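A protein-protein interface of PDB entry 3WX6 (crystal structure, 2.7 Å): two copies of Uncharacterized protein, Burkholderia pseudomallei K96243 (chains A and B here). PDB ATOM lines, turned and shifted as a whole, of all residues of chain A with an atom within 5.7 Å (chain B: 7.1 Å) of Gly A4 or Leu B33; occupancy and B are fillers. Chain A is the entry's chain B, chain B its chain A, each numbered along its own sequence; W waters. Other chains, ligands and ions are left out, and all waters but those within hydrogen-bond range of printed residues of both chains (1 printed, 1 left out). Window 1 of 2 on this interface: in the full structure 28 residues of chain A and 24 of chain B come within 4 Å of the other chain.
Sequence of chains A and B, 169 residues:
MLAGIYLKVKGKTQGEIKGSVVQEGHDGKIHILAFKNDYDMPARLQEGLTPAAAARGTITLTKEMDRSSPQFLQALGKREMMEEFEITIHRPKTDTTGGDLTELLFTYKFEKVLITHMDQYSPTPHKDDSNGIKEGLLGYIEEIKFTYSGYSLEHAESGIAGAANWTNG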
ATOM      1  N   ALA A   3      29.842 -17.924   0.106  1.00  0.00           N
ATOM      2  CA  ALA A   3      30.390 -17.163  -1.010  1.00  0.00           C
ATOM      3  C   ALA A   3      29.541 -17.294  -2.263  1.00  0.00           C
ATOM      4  O   ALA A   3      28.363 -17.657  -2.204  1.00  0.00           O
ATOM      5  CB  ALA A   3      31.812 -17.603  -1.309  1.00  0.00           C
ATOM      6  N   GLY A   4      30.155 -16.987  -3.399  1.00  0.00           N
ATOM      7  CA  GLY A   4      29.494 -17.086  -4.686  1.00  0.00           C
ATOM      8  C   GLY A   4      29.956 -18.322  -5.431  1.00  0.00           C
ATOM      9  O   GLY A   4      29.669 -19.441  -5.002  1.00  0.00           O
ATOM     10  N   ILE A   5      30.665 -18.121  -6.542  1.00  0.00           N
ATOM     11  CA  ILE A   5      31.255 -19.228  -7.290  1.00  0.00           C
ATOM     12  C   ILE A   5      32.762 -19.099  -7.427  1.00  0.00           C
ATOM     13  O   ILE A   5      33.264 -18.005  -7.653  1.00  0.00           O
ATOM     14  CB  ILE A   5      30.643 -19.360  -8.716  1.00  0.00           C
ATOM     15  CG1 ILE A   5      31.090 -20.674  -9.355  1.00  0.00           C
ATOM     16  CG2 ILE A   5      31.001 -18.188  -9.617  1.00  0.00           C
ATOM     17  CD1 ILE A   5      30.507 -20.904 -10.702  1.00  0.00           C
ATOM     18  N   TYR A   6      33.483 -20.208  -7.252  1.00  0.00           N
ATOM     19  CA  TYR A   6      34.836 -20.321  -7.795  1.00  0.00           C
ATOM     20  C   TYR A   6      34.721 -21.015  -9.142  1.00  0.00           C
ATOM     21  O   TYR A   6      34.221 -22.132  -9.239  1.00  0.00           O
ATOM     22  CB  TYR A   6      35.804 -21.070  -6.864  1.00  0.00           C
ATOM     23  CG  TYR A   6      36.408 -20.216  -5.759  1.00  0.00           C
ATOM     24  CD1 TYR A   6      35.608 -19.471  -4.903  1.00  0.00           C
ATOM     25  CD2 TYR A   6      37.789 -20.121  -5.609  1.00  0.00           C
ATOM     26  CE1 TYR A   6      36.166 -18.679  -3.905  1.00  0.00           C
ATOM     27  CE2 TYR A   6      38.357 -19.330  -4.615  1.00  0.00           C
ATOM     28  CZ  TYR A   6      37.539 -18.612  -3.767  1.00  0.00           C
ATOM     29  OH  TYR A   6      38.103 -17.828  -2.785  1.00  0.00           O
ATOM     30  N   GLY A  19      35.632 -14.588  -4.864  1.00  0.00           N
ATOM     31  CA  GLY A  19      34.547 -15.462  -5.291  1.00  0.00           C
ATOM     32  C   GLY A  19      33.337 -14.691  -5.784  1.00  0.00           C
ATOM     33  O   GLY A  19      32.923 -13.700  -5.177  1.00  0.00           O
ATOM     34  N   SER A  20      32.759 -15.153  -6.884  1.00  0.00           N
ATOM     35  CA  SER A  20      31.698 -14.406  -7.532  1.00  0.00           C
ATOM     36  C   SER A  20      30.350 -14.652  -6.869  1.00  0.00           C
ATOM     37  O   SER A  20      29.977 -13.933  -5.950  1.00  0.00           O
ATOM     38  CB  SER A  20      31.648 -14.758  -9.016  1.00  0.00           C
ATOM     39  OG  SER A  20      30.696 -13.960  -9.688  1.00  0.00           O
ATOM     40  N   PHE A  35      20.672 -17.933  -7.056  1.00  0.00           N
ATOM     41  CA  PHE A  35      20.821 -19.263  -7.635  1.00  0.00           C
ATOM     42  C   PHE A  35      19.588 -20.141  -7.421  1.00  0.00           C
ATOM     43  O   PHE A  35      19.016 -20.156  -6.336  1.00  0.00           O
ATOM     44  CB  PHE A  35      22.045 -19.951  -7.062  1.00  0.00           C
ATOM     45  N   LEU A  61      21.804 -19.066 -12.006  1.00  0.00           N
ATOM     46  CA  LEU A  61      22.475 -18.126 -11.111  1.00  0.00           C
ATOM     47  C   LEU A  61      22.041 -16.703 -11.441  1.00  0.00           C
ATOM     48  O   LEU A  61      22.016 -16.325 -12.611  1.00  0.00           O
ATOM     49  CB  LEU A  61      24.002 -18.247 -11.247  1.00  0.00           C
ATOM     50  CG  LEU A  61      24.772 -19.522 -10.872  1.00  0.00           C
ATOM     51  CD1 LEU A  61      26.279 -19.286 -10.970  1.00  0.00           C
ATOM     52  CD2 LEU A  61      24.411 -20.001  -9.492  1.00  0.00           C
ATOM     53  N   THR A  62      21.667 -15.921 -10.433  1.00  0.00           N
ATOM     54  CA  THR A  62      21.413 -14.495 -10.655  1.00  0.00           C
ATOM     55  C   THR A  62      22.549 -13.659 -10.062  1.00  0.00           C
ATOM     56  O   THR A  62      23.085 -14.010  -9.015  1.00  0.00           O
ATOM     57  CB  THR A  62      20.069 -14.041 -10.040  1.00  0.00           C
ATOM     58  OG1 THR A  62      20.136 -14.143  -8.615  1.00  0.00           O
ATOM     59  CG2 THR A  62      18.926 -14.899 -10.547  1.00  0.00           C
ATOM     60  N   LYS A  63      22.947 -12.590 -10.753  1.00  0.00           N
ATOM     61  CA  LYS A  63      24.028 -11.720 -10.273  1.00  0.00           C
ATOM     62  C   LYS A  63      24.003 -10.397 -11.041  1.00  0.00           C
ATOM     63  O   LYS A  63      23.373 -10.320 -12.082  1.00  0.00           O
ATOM     64  CB  LYS A  63      25.394 -12.395 -10.442  1.00  0.00           C
ATOM     65  CG  LYS A  63      25.961 -12.311 -11.857  1.00  0.00           C
ATOM     66  CD  LYS A  63      27.342 -12.949 -11.966  1.00  0.00           C
ATOM     67  CE  LYS A  63      28.079 -12.489 -13.221  1.00  0.00           C
ATOM     68  NZ  LYS A  63      27.160 -12.217 -14.360  1.00  0.00           N
ATOM     69  N   GLU A  86      32.154 -24.588  -8.655  1.00  0.00           N
ATOM     70  CA  GLU A  86      31.732 -24.835  -7.287  1.00  0.00           C
ATOM     71  C   GLU A  86      31.071 -23.584  -6.710  1.00  0.00           C
ATOM     72  O   GLU A  86      31.653 -22.497  -6.728  1.00  0.00           O
ATOM     73  CB  GLU A  86      32.920 -25.321  -6.430  1.00  0.00           C
ATOM     74  CG  GLU A  86      33.563 -24.304  -5.480  1.00  0.00           C
ATOM     75  CD  GLU A  86      34.484 -24.952  -4.460  1.00  0.00           C
ATOM     76  OE1 GLU A  86      35.089 -25.999  -4.783  1.00  0.00           O
ATOM     77  OE2 GLU A  86      34.595 -24.418  -3.335  1.00  0.00           O
ATOM     78  N   ILE A  87      29.819 -23.715  -6.277  1.00  0.00           N
ATOM     79  CA  ILE A  87      29.158 -22.560  -5.690  1.00  0.00           C
ATOM     80  C   ILE A  87      28.960 -22.941  -4.216  1.00  0.00           C
ATOM     81  O   ILE A  87      28.206 -23.855  -3.868  1.00  0.00           O
ATOM     82  CB  ILE A  87      27.841 -22.107  -6.473  1.00  0.00           C
ATOM     83  CG1 ILE A  87      26.862 -23.213  -6.835  1.00  0.00           C
ATOM     84  CG2 ILE A  87      28.165 -21.458  -7.776  1.00  0.00           C
ATOM     85  CD1 ILE A  87      25.898 -23.517  -5.773  1.00  0.00           C
ATOM     86  N   THR A  88      29.697 -22.240  -3.358  1.00  0.00           N
ATOM     87  CA  THR A  88      29.730 -22.526  -1.927  1.00  0.00           C
ATOM     88  C   THR A  88      28.891 -21.541  -1.126  1.00  0.00           C
ATOM     89  O   THR A  88      28.794 -20.355  -1.447  1.00  0.00           O
ATOM     90  CB  THR A  88      31.180 -22.539  -1.397  1.00  0.00           C
ATOM     91  OG1 THR A  88      31.195 -22.950  -0.025  1.00  0.00           O
ATOM     92  CG2 THR A  88      31.805 -21.168  -1.513  1.00  0.00           C
ATOM     93  N   LEU B   7      30.558 -13.607  -3.780  1.00  0.00           N
ATOM     94  CA  LEU B   7      30.559 -12.978  -2.461  1.00  0.00           C
ATOM     95  C   LEU B   7      31.762 -13.332  -1.643  1.00  0.00           C
ATOM     96  O   LEU B   7      31.936 -14.488  -1.292  1.00  0.00           O
ATOM     97  CB  LEU B   7      29.322 -13.367  -1.644  1.00  0.00           C
ATOM     98  CG  LEU B   7      29.253 -12.714  -0.247  1.00  0.00           C
ATOM     99  CD1 LEU B   7      29.526 -11.213  -0.270  1.00  0.00           C
ATOM    100  CD2 LEU B   7      27.944 -12.988   0.466  1.00  0.00           C
ATOM    101  N   LYS B   8      32.582 -12.344  -1.307  1.00  0.00           N
ATOM    102  CA  LYS B   8      33.614 -12.599  -0.321  1.00  0.00           C
ATOM    103  C   LYS B   8      33.105 -11.881   0.917  1.00  0.00           C
ATOM    104  O   LYS B   8      32.921 -10.663   0.912  1.00  0.00           O
ATOM    105  CB  LYS B   8      34.986 -12.088  -0.779  1.00  0.00           C
ATOM    106  CG  LYS B   8      36.155 -12.678   0.000  1.00  0.00           C
ATOM    107  CD  LYS B   8      37.264 -11.661   0.223  1.00  0.00           C
ATOM    108  CE  LYS B   8      38.315 -12.179   1.194  1.00  0.00           C
ATOM    109  NZ  LYS B   8      38.944 -13.461   0.767  1.00  0.00           N
ATOM    110  N   ILE B  32      26.361 -17.907  -3.468  1.00  0.00           N
ATOM    111  CA  ILE B  32      26.281 -18.592  -4.750  1.00  0.00           C
ATOM    112  C   ILE B  32      25.616 -17.712  -5.793  1.00  0.00           C
ATOM    113  O   ILE B  32      24.554 -18.063  -6.319  1.00  0.00           O
ATOM    114  CB  ILE B  32      25.496 -19.907  -4.642  1.00  0.00           C
ATOM    115  N   LEU B  33      26.256 -16.582  -6.092  1.00  0.00           N
ATOM    116  CA  LEU B  33      25.724 -15.602  -7.030  1.00  0.00           C
ATOM    117  C   LEU B  33      24.380 -15.089  -6.533  1.00  0.00           C
ATOM    118  O   LEU B  33      23.376 -15.783  -6.657  1.00  0.00           O
ATOM    119  CB  LEU B  33      25.585 -16.205  -8.432  1.00  0.00           C
ATOM    120  N   ALA B  34      24.372 -13.878  -5.973  1.00  0.00           N
ATOM    121  CA  ALA B  34      23.154 -13.257  -5.434  1.00  0.00           C
ATOM    122  C   ALA B  34      22.048 -13.115  -6.480  1.00  0.00           C
ATOM    123  O   ALA B  34      21.429 -14.114  -6.816  1.00  0.00           O
ATOM    124  N   PHE B  35      21.707 -11.907  -6.950  1.00  0.00           N
ATOM    125  CA  PHE B  35      21.880 -10.603  -6.289  1.00  0.00           C
ATOM    126  C   PHE B  35      21.033  -9.568  -7.040  1.00  0.00           C
ATOM    127  O   PHE B  35      21.089  -9.493  -8.264  1.00  0.00           O
ATOM    128  CB  PHE B  35      23.335 -10.134  -6.250  1.00  0.00           C
ATOM    129  N   LEU B  61      20.596 -10.957  -2.021  1.00  0.00           N
ATOM    130  CA  LEU B  61      21.301 -12.070  -2.643  1.00  0.00           C
ATOM    131  C   LEU B  61      20.498 -13.352  -2.520  1.00  0.00           C
ATOM    132  O   LEU B  61      20.071 -13.717  -1.424  1.00  0.00           O
ATOM    133  CB  LEU B  61      22.689 -12.274  -2.012  1.00  0.00           C
ATOM    134  CG  LEU B  61      23.855 -11.286  -2.172  1.00  0.00           C
ATOM    135  CD1 LEU B  61      23.553  -9.915  -1.633  1.00  0.00           C
ATOM    136  CD2 LEU B  61      25.112 -11.846  -1.517  1.00  0.00           C
ATOM    137  N   THR B  62      20.289 -14.040  -3.639  1.00  0.00           N
ATOM    138  CA  THR B  62      19.694 -15.371  -3.571  1.00  0.00           C
ATOM    139  C   THR B  62      20.776 -16.395  -3.864  1.00  0.00           C
ATOM    140  O   THR B  62      21.646 -16.176  -4.706  1.00  0.00           O
ATOM    141  CB  THR B  62      18.480 -15.554  -4.533  1.00  0.00           C
ATOM    142  OG1 THR B  62      17.856 -16.821  -4.284  1.00  0.00           O
ATOM    143  CG2 THR B  62      18.892 -15.482  -5.984  1.00  0.00           C
ATOM    144  N   LYS B  63      20.722 -17.498  -3.128  1.00  0.00           N
ATOM    145  CA  LYS B  63      21.708 -18.566  -3.217  1.00  0.00           C
ATOM    146  C   LYS B  63      21.109 -19.795  -2.546  1.00  0.00           C
ATOM    147  O   LYS B  63      20.053 -19.692  -1.921  1.00  0.00           O
ATOM    148  CB  LYS B  63      23.025 -18.130  -2.567  1.00  0.00           C
ATOM    149  CG  LYS B  63      23.077 -18.314  -1.053  1.00  0.00           C
ATOM    150  CD  LYS B  63      24.284 -17.599  -0.468  1.00  0.00           C
ATOM    151  CE  LYS B  63      24.594 -18.052   0.951  1.00  0.00           C
ATOM    152  NZ  LYS B  63      23.372 -18.299   1.759  1.00  0.00           N
ATOM    153  N   GLU B  64      21.748 -20.954  -2.671  1.00  0.00           N
ATOM    154  CA  GLU B  64      21.244 -22.122  -1.957  1.00  0.00           C
ATOM    155  C   GLU B  64      21.489 -22.040  -0.447  1.00  0.00           C
ATOM    156  O   GLU B  64      21.520 -20.954   0.124  1.00  0.00           O
ATOM    157  CB  GLU B  64      21.840 -23.421  -2.505  1.00  0.00           C
ATOM    158  CG  GLU B  64      21.282 -23.909  -3.846  1.00  0.00           C
ATOM    159  CD  GLU B  64      21.430 -22.931  -4.994  1.00  0.00           C
ATOM    160  OE1 GLU B  64      21.919 -21.804  -4.786  1.00  0.00           O
ATOM    161  OE2 GLU B  64      21.050 -23.304  -6.125  1.00  0.00           O
ATOM    162  N   ILE B  87      31.420  -8.027  -3.596  1.00  0.00           N
ATOM    163  CA  ILE B  87      30.733  -8.834  -4.583  1.00  0.00           C
ATOM    164  C   ILE B  87      31.422  -8.664  -5.933  1.00  0.00           C
ATOM    165  O   ILE B  87      31.458  -7.558  -6.476  1.00  0.00           O
ATOM    166  CB  ILE B  87      29.240  -8.435  -4.696  1.00  0.00           C
ATOM    167  CG1 ILE B  87      28.403  -9.036  -3.557  1.00  0.00           C
ATOM    168  CG2 ILE B  87      28.664  -8.886  -6.019  1.00  0.00           C
ATOM    169  CD1 ILE B  87      28.232 -10.536  -3.629  1.00  0.00           C
ATOM    170  N   THR B  88      32.024  -9.732  -6.451  1.00  0.00           N
ATOM    171  CA  THR B  88      32.673  -9.651  -7.758  1.00  0.00           C
ATOM    172  C   THR B  88      31.699 -10.276  -8.738  1.00  0.00           C
ATOM    173  O   THR B  88      31.056 -11.284  -8.445  1.00  0.00           O
ATOM    174  CB  THR B  88      34.057 -10.341  -7.791  1.00  0.00           C
ATOM    175  OG1 THR B  88      34.673 -10.137  -9.069  1.00  0.00           O
ATOM    176  CG2 THR B  88      33.938 -11.802  -7.539  1.00  0.00           C
ATOM    177  N   ILE B  89      31.568  -9.646  -9.895  1.00  0.00           N
ATOM    178  CA  ILE B  89      30.356  -9.819 -10.665  1.00  0.00           C
ATOM    179  C   ILE B  89      30.540  -9.712 -12.173  1.00  0.00           C
ATOM    180  O   ILE B  89      31.490 -10.251 -12.726  1.00  0.00           O
ATOM    181  CB  ILE B  89      29.310  -8.782 -10.168  1.00  0.00           C
ATOM    182  CG1 ILE B  89      27.931  -9.418 -10.031  1.00  0.00           C
ATOM    183  CG2 ILE B  89      29.338  -7.513 -10.975  1.00  0.00           C
ATOM    184  CD1 ILE B  89      27.936 -10.567  -9.071  1.00  0.00           C
HETATM  185  O   HOH W   1      27.357 -12.854  -6.201  1.00  0.00           O
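The backbone carbonyl oxygen (O) of Ser A20 lies close to the backbone NH (N) of Leu B7, at 2.3 Å.
The backbone carbonyl oxygen of Leu B33 is in hydrogen-bond range of the backbone NH of Phe A35 (3.5 Å).
O of Gly A19 sits at hydrogen-bond distance from N of Leu B7 (2.7 Å).
N of Gly A4 lies close to N of Leu B7, 3.4 Å away.
The backbone carbonyl oxygen of Leu B33 lies close to the backbone carbonyl oxygen of Thr A62 (3.0 Å).
The side-chain hydroxyl (OG1) of Thr A62 lies within hydrogen-bond range of the backbone NH (N) of Phe B35, at 3.2 Å.
The backbone carbonyl oxygen (O) of Thr B88 is in hydrogen-bond range of the side-chain hydroxyl (OG) of Ser A20, at 3.0 Å.
N of Phe A35 is in hydrogen-bond range of O of Thr B62 (3.1 Å).
The backbone NH (N) of Ile B32 sits close to the backbone carbonyl oxygen (O) of Ala A3 (2.4 Å).
The backbone NH (N) of Ala B34 sits close to the backbone carbonyl oxygen (O) of Thr A62 (3.3 Å).
Gly A4 touches just these residues of chain B: Leu B7 (3.4 Å), Ile B32 (3.5 Å) and Leu B33 (3.6 Å).
Printed residues of chain B within 4 Å of Leu A61: Ile B32 and Leu B33.
Of the printed residues of chain B, Thr A88 touches Ile B32 (3.9996 Å).
Leu B33 touches just these residues of chain A: Gly A4 (3.6 Å), Phe A35 (3.5 Å), Leu A61 (3.8 Å) and Thr A62 (3.0 Å).
Of the printed residues of chain A, Lys B63 touches Phe A35 (3.95 Å).
Of the printed residues of chain A, Glu B64 touches Phe A35 (2.9 Å).
The nearest residue of chain A that does not touch Leu B33 is Lys A63 (4.3 Å).
The nearest printed residue of chain A that does not touch Ile B32 is Ile A5 (4.8 Å).
Water W1 bridges the backbone carbonyl oxygen of Ser A20 and the backbone NH of Ala B34.
Printed residues of chain B that touch a printed residue of chain A: Leu B7, Ile B32, Leu B33, Ala B34, Phe B35, Thr B62, Lys B63, Glu B64, Thr B88 and Ile B89.
Hydrophobic or aromatic side chains of chain B that line the printed part of chain A: Leu B7, Ile B32, Leu B33 and Ile B89.
Among the printed residues, 24 pairs touch across the chains.
Phe A35 touches Thr B62, and with the chains exchanged Thr A62 touches Phe B35.
Phe A35 touches Lys B63, but with the chains exchanged Lys A63 does not touch Phe B35 (4.1 Å).
Thr B62 touches its own counterpart, Thr A62.
6 positions are printed for both chains.
Of the 24 pairs that touch across the chains among the printed residues, 3 have their exchanged pair printed and touching as well.
The backbone carbonyl oxygen (O) of Ala B34 sits close to the backbone NH (N) of Thr B62 (3.4 Å).
N of Ala A3 lies within hydrogen-bond range of O of Thr A88, 3.1 Å away.
O of Leu B33 sits close to O of Thr B62, 2.6 Å away.
The backbone NH (N) of Ser A20 sits at hydrogen-bond distance from the backbone carbonyl oxygen (O) of Ile A5 (3.0 Å).
N of Thr A88 is in hydrogen-bond range of O of Gly A4, 3.2 Å away.
Among the printed residues, merely in contact across the chains: Ala A3 with Leu B7, Gly A4 with Ile B32, Gly A4 with Leu B33, Gly A19 with Thr B88, Phe A35 with Ile B32, Phe A35 with Ala B34, Phe A35 with Lys B63, Phe A35 with Glu B64, Leu A61 with Ile B32, Leu A61 with Leu B33, Thr A62 with Thr B62, Lys A63 with Ile B89, Ile A87 with Ile B32 and Thr A88 with Ile B32.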
